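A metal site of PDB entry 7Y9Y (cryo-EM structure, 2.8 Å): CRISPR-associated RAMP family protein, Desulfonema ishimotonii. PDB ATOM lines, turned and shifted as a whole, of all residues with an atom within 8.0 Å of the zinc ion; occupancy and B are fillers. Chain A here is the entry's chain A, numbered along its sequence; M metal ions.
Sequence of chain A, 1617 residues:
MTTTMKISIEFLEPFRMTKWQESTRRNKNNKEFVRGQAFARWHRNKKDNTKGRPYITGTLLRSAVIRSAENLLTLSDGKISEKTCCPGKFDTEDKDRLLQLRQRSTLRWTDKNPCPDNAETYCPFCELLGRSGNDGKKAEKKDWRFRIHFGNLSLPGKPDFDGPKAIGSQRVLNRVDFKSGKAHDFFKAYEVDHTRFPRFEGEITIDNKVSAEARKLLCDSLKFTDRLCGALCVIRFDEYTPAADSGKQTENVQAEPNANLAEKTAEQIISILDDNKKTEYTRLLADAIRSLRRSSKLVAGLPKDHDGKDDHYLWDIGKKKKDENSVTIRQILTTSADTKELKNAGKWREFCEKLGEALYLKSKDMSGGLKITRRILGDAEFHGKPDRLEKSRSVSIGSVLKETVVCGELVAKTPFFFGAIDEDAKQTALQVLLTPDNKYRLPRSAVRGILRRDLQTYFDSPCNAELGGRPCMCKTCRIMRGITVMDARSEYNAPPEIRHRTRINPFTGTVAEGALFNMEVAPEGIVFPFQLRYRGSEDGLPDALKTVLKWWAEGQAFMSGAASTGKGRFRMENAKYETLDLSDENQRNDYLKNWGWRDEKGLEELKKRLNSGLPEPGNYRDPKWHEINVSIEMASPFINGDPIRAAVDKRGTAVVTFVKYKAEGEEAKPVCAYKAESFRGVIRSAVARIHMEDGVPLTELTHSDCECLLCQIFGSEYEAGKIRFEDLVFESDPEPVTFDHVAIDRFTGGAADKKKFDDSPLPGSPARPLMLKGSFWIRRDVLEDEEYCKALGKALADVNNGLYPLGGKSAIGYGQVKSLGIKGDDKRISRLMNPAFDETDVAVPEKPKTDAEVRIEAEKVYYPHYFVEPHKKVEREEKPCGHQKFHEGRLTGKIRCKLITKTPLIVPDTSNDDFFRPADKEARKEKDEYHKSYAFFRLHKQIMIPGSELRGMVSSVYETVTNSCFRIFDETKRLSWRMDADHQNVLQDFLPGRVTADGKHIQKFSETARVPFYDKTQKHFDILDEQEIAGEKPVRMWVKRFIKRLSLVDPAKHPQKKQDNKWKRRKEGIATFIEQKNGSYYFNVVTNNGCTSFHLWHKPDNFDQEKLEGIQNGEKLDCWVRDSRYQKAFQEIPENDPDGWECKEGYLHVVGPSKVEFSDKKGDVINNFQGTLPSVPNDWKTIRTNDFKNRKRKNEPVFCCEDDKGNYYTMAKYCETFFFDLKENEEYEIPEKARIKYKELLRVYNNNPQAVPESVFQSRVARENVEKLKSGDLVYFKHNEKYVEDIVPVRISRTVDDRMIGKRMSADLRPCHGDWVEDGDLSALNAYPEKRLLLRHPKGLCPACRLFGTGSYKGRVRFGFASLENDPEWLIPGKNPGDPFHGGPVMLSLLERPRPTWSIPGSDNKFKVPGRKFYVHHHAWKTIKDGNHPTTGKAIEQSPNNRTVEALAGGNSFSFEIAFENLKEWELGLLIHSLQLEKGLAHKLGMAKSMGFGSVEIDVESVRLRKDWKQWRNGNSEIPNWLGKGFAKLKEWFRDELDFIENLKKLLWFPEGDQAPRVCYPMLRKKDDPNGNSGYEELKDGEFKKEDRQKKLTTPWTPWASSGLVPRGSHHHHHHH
The guanidinium group (NH1) of Arg 452 sits close to the side-chain sulfur (SG) of Cys 477, 3.4 Å away.
The backbone NH of Ala 465 sits close to the side-chain sulfur of Cys 463, at 3.7 Å.
The backbone NH (N) of Cys 463 sits at hydrogen-bond distance from the side-chain amide oxygen (OE1) of Gln 456 (3.2 Å).
The backbone carbonyl oxygen (O) of Cys 472 sits at hydrogen-bond distance from the guanidinium group (NH1) of Arg 481, 2.6 Å away.
The zinc ion is bound by the side-chain sulfur (SG) of Cys 477 (2.3 Å), the side-chain sulfur (SG) of Cys 472 (2.3 Å), the side-chain sulfur (SG) of Cys 463 (2.3 Å) and the side-chain sulfur (SG) of Cys 474 (2.3 Å).
The nearest printed residue that does not touch the zinc ion is Ala 465 (4.3 Å).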
ATOM      1  N   ARG A 452      -5.801   4.670  -6.466  1.00  0.00           N
ATOM      2  CA  ARG A 452      -5.095   5.847  -5.980  1.00  0.00           C
ATOM      3  C   ARG A 452      -3.630   5.527  -5.670  1.00  0.00           C
ATOM      4  O   ARG A 452      -2.732   6.290  -6.033  1.00  0.00           O
ATOM      5  CB  ARG A 452      -5.799   6.400  -4.738  1.00  0.00           C
ATOM      6  CG  ARG A 452      -5.233   7.688  -4.199  1.00  0.00           C
ATOM      7  CD  ARG A 452      -6.055   8.201  -3.030  1.00  0.00           C
ATOM      8  NE  ARG A 452      -7.328   8.762  -3.471  1.00  0.00           N
ATOM      9  CZ  ARG A 452      -7.476  10.010  -3.920  1.00  0.00           C
ATOM     10  NH1 ARG A 452      -6.452  10.836  -4.006  1.00  0.00           N
ATOM     11  NH2 ARG A 452      -8.683  10.424  -4.287  1.00  0.00           N
ATOM     12  N   GLN A 456      -0.370   7.109  -7.615  1.00  0.00           N
ATOM     13  CA  GLN A 456       0.729   7.726  -6.891  1.00  0.00           C
ATOM     14  C   GLN A 456       2.058   7.055  -7.187  1.00  0.00           C
ATOM     15  O   GLN A 456       3.089   7.742  -7.269  1.00  0.00           O
ATOM     16  CB  GLN A 456       0.455   7.696  -5.398  1.00  0.00           C
ATOM     17  CG  GLN A 456      -0.532   8.735  -4.919  1.00  0.00           C
ATOM     18  CD  GLN A 456      -1.038   8.450  -3.530  1.00  0.00           C
ATOM     19  OE1 GLN A 456      -0.661   9.122  -2.570  1.00  0.00           O
ATOM     20  NE2 GLN A 456      -1.898   7.450  -3.413  1.00  0.00           N
ATOM     21  N   SER A 461       4.918  10.589  -6.753  1.00  0.00           N
ATOM     22  CA  SER A 461       4.701  11.654  -5.803  1.00  0.00           C
ATOM     23  C   SER A 461       3.553  11.296  -4.874  1.00  0.00           C
ATOM     24  O   SER A 461       2.419  11.128  -5.322  1.00  0.00           O
ATOM     25  CB  SER A 461       4.376  12.971  -6.533  1.00  0.00           C
ATOM     26  OG  SER A 461       5.087  13.069  -7.755  1.00  0.00           O
ATOM     27  N   PRO A 462       3.802  11.172  -3.562  1.00  0.00           N
ATOM     28  CA  PRO A 462       2.703  11.007  -2.622  1.00  0.00           C
ATOM     29  C   PRO A 462       1.812  12.238  -2.589  1.00  0.00           C
ATOM     30  O   PRO A 462       2.255  13.353  -2.868  1.00  0.00           O
ATOM     31  CB  PRO A 462       3.407  10.796  -1.280  1.00  0.00           C
ATOM     32  CG  PRO A 462       4.773  10.312  -1.647  1.00  0.00           C
ATOM     33  CD  PRO A 462       5.110  11.028  -2.908  1.00  0.00           C
ATOM     34  N   CYS A 463       0.546  12.019  -2.255  1.00  0.00           N
ATOM     35  CA  CYS A 463      -0.428  13.099  -2.141  1.00  0.00           C
ATOM     36  C   CYS A 463      -0.548  13.506  -0.690  1.00  0.00           C
ATOM     37  O   CYS A 463      -1.074  12.742   0.129  1.00  0.00           O
ATOM     38  CB  CYS A 463      -1.788  12.662  -2.699  1.00  0.00           C
ATOM     39  SG  CYS A 463      -3.147  13.737  -2.215  1.00  0.00           S
ATOM     40  N   ASN A 464      -0.044  14.687  -0.360  1.00  0.00           N
ATOM     41  CA  ASN A 464      -0.085  15.208   1.011  1.00  0.00           C
ATOM     42  C   ASN A 464      -1.332  16.034   1.251  1.00  0.00           C
ATOM     43  O   ASN A 464      -1.277  17.179   1.712  1.00  0.00           O
ATOM     44  CB  ASN A 464       1.179  16.020   1.295  1.00  0.00           C
ATOM     45  CG  ASN A 464       2.447  15.223   1.077  1.00  0.00           C
ATOM     46  OD1 ASN A 464       2.816  14.372   1.889  1.00  0.00           O
ATOM     47  ND2 ASN A 464       3.127  15.497  -0.031  1.00  0.00           N
ATOM     48  N   ALA A 465      -2.490  15.462   0.943  1.00  0.00           N
ATOM     49  CA  ALA A 465      -3.750  16.131   1.222  1.00  0.00           C
ATOM     50  C   ALA A 465      -4.241  15.769   2.619  1.00  0.00           C
ATOM     51  O   ALA A 465      -3.817  14.781   3.226  1.00  0.00           O
ATOM     52  CB  ALA A 465      -4.806  15.745   0.181  1.00  0.00           C
ATOM     53  N   GLU A 466      -5.156  16.586   3.128  1.00  0.00           N
ATOM     54  CA  GLU A 466      -5.797  16.343   4.407  1.00  0.00           C
ATOM     55  C   GLU A 466      -7.301  16.381   4.224  1.00  0.00           C
ATOM     56  O   GLU A 466      -7.822  17.081   3.341  1.00  0.00           O
ATOM     57  CB  GLU A 466      -5.373  17.362   5.467  1.00  0.00           C
ATOM     58  CG  GLU A 466      -4.534  16.783   6.600  1.00  0.00           C
ATOM     59  CD  GLU A 466      -5.257  15.680   7.345  1.00  0.00           C
ATOM     60  OE1 GLU A 466      -6.465  15.836   7.635  1.00  0.00           O
ATOM     61  OE2 GLU A 466      -4.610  14.649   7.653  1.00  0.00           O
ATOM     62  N   PRO A 471     -10.499  21.109  -2.675  1.00  0.00           N
ATOM     63  CA  PRO A 471     -10.040  19.871  -3.314  1.00  0.00           C
ATOM     64  C   PRO A 471      -8.563  19.925  -3.670  1.00  0.00           C
ATOM     65  O   PRO A 471      -8.051  20.950  -4.102  1.00  0.00           O
ATOM     66  CB  PRO A 471     -10.909  19.778  -4.573  1.00  0.00           C
ATOM     67  CG  PRO A 471     -12.141  20.524  -4.218  1.00  0.00           C
ATOM     68  CD  PRO A 471     -11.672  21.670  -3.360  1.00  0.00           C
ATOM     69  N   CYS A 472      -7.881  18.795  -3.466  1.00  0.00           N
ATOM     70  CA  CYS A 472      -6.474  18.701  -3.815  1.00  0.00           C
ATOM     71  C   CYS A 472      -6.295  18.707  -5.324  1.00  0.00           C
ATOM     72  O   CYS A 472      -7.098  18.136  -6.076  1.00  0.00           O
ATOM     73  CB  CYS A 472      -5.867  17.425  -3.208  1.00  0.00           C
ATOM     74  SG  CYS A 472      -4.086  17.287  -3.387  1.00  0.00           S
ATOM     75  N   MET A 473      -5.224  19.345  -5.785  1.00  0.00           N
ATOM     76  CA  MET A 473      -5.007  19.571  -7.206  1.00  0.00           C
ATOM     77  C   MET A 473      -3.757  18.877  -7.725  1.00  0.00           C
ATOM     78  O   MET A 473      -3.149  19.344  -8.687  1.00  0.00           O
ATOM     79  CB  MET A 473      -4.941  21.070  -7.514  1.00  0.00           C
ATOM     80  CG  MET A 473      -6.123  21.856  -6.960  1.00  0.00           C
ATOM     81  SD  MET A 473      -7.555  21.822  -8.047  1.00  0.00           S
ATOM     82  CE  MET A 473      -6.765  21.858  -9.657  1.00  0.00           C
ATOM     83  N   CYS A 474      -3.340  17.778  -7.102  1.00  0.00           N
ATOM     84  CA  CYS A 474      -2.268  16.982  -7.687  1.00  0.00           C
ATOM     85  C   CYS A 474      -2.844  16.106  -8.790  1.00  0.00           C
ATOM     86  O   CYS A 474      -4.053  15.915  -8.924  1.00  0.00           O
ATOM     87  CB  CYS A 474      -1.584  16.135  -6.619  1.00  0.00           C
ATOM     88  SG  CYS A 474      -2.615  14.879  -5.843  1.00  0.00           S
ATOM     89  N   LYS A 475      -1.944  15.544  -9.606  1.00  0.00           N
ATOM     90  CA  LYS A 475      -2.376  14.744 -10.753  1.00  0.00           C
ATOM     91  C   LYS A 475      -3.174  13.535 -10.305  1.00  0.00           C
ATOM     92  O   LYS A 475      -4.155  13.147 -10.958  1.00  0.00           O
ATOM     93  CB  LYS A 475      -1.162  14.324 -11.582  1.00  0.00           C
ATOM     94  CG  LYS A 475      -0.455  15.472 -12.272  1.00  0.00           C
ATOM     95  CD  LYS A 475       1.042  15.230 -12.348  1.00  0.00           C
ATOM     96  CE  LYS A 475       1.676  15.128 -10.971  1.00  0.00           C
ATOM     97  NZ  LYS A 475       1.098  16.087  -9.998  1.00  0.00           N
ATOM     98  N   THR A 476      -2.791  12.917  -9.192  1.00  0.00           N
ATOM     99  CA  THR A 476      -3.528  11.779  -8.665  1.00  0.00           C
ATOM    100  C   THR A 476      -4.955  12.161  -8.313  1.00  0.00           C
ATOM    101  O   THR A 476      -5.901  11.477  -8.708  1.00  0.00           O
ATOM    102  CB  THR A 476      -2.814  11.207  -7.439  1.00  0.00           C
ATOM    103  OG1 THR A 476      -1.399  11.232  -7.640  1.00  0.00           O
ATOM    104  CG2 THR A 476      -3.265   9.783  -7.173  1.00  0.00           C
ATOM    105  N   CYS A 477      -5.139  13.271  -7.595  1.00  0.00           N
ATOM    106  CA  CYS A 477      -6.486  13.692  -7.218  1.00  0.00           C
ATOM    107  C   CYS A 477      -7.284  14.154  -8.431  1.00  0.00           C
ATOM    108  O   CYS A 477      -8.495  13.910  -8.500  1.00  0.00           O
ATOM    109  CB  CYS A 477      -6.420  14.783  -6.157  1.00  0.00           C
ATOM    110  SG  CYS A 477      -6.067  14.183  -4.491  1.00  0.00           S
ATOM    111  N   ARG A 478      -6.634  14.829  -9.376  1.00  0.00           N
ATOM    112  CA  ARG A 478      -7.339  15.245 -10.588  1.00  0.00           C
ATOM    113  C   ARG A 478      -7.860  14.045 -11.369  1.00  0.00           C
ATOM    114  O   ARG A 478      -8.986  14.075 -11.883  1.00  0.00           O
ATOM    115  CB  ARG A 478      -6.439  16.113 -11.473  1.00  0.00           C
ATOM    116  CG  ARG A 478      -6.253  17.535 -10.981  1.00  0.00           C
ATOM    117  CD  ARG A 478      -4.805  17.972 -11.109  1.00  0.00           C
ATOM    118  NE  ARG A 478      -4.667  19.416 -11.241  1.00  0.00           N
ATOM    119  CZ  ARG A 478      -3.541  20.035 -11.557  1.00  0.00           C
ATOM    120  NH1 ARG A 478      -2.426  19.363 -11.792  1.00  0.00           N
ATOM    121  NH2 ARG A 478      -3.531  21.365 -11.653  1.00  0.00           N
ATOM    122  N   MET A 480      -8.437  11.040 -10.038  1.00  0.00           N
ATOM    123  CA  MET A 480      -9.380  10.318  -9.196  1.00  0.00           C
ATOM    124  C   MET A 480     -10.741  10.991  -9.149  1.00  0.00           C
ATOM    125  O   MET A 480     -11.749  10.315  -8.927  1.00  0.00           O
ATOM    126  CB  MET A 480      -8.816  10.158  -7.784  1.00  0.00           C
ATOM    127  CG  MET A 480      -7.789   9.056  -7.645  1.00  0.00           C
ATOM    128  SD  MET A 480      -8.287   7.559  -8.501  1.00  0.00           S
ATOM    129  CE  MET A 480      -9.009   6.624  -7.165  1.00  0.00           C
ATOM    130  N   ARG A 481     -10.796  12.309  -9.324  1.00  0.00           N
ATOM    131  CA  ARG A 481     -12.069  13.004  -9.280  1.00  0.00           C
ATOM    132  C   ARG A 481     -12.952  12.693 -10.483  1.00  0.00           C
ATOM    133  O   ARG A 481     -14.155  12.967 -10.437  1.00  0.00           O
ATOM    134  CB  ARG A 481     -11.853  14.512  -9.180  1.00  0.00           C
ATOM    135  CG  ARG A 481     -11.599  14.988  -7.757  1.00  0.00           C
ATOM    136  CD  ARG A 481     -11.886  16.462  -7.605  1.00  0.00           C
ATOM    137  NE  ARG A 481     -10.839  17.284  -8.185  1.00  0.00           N
ATOM    138  CZ  ARG A 481      -9.751  17.683  -7.537  1.00  0.00           C
ATOM    139  NH1 ARG A 481      -9.539  17.326  -6.279  1.00  0.00           N
ATOM    140  NH2 ARG A 481      -8.867  18.445  -8.155  1.00  0.00           N
HETATM  141 ZN    ZN M   1      -3.977  15.039  -3.958  1.00  0.00          ZN
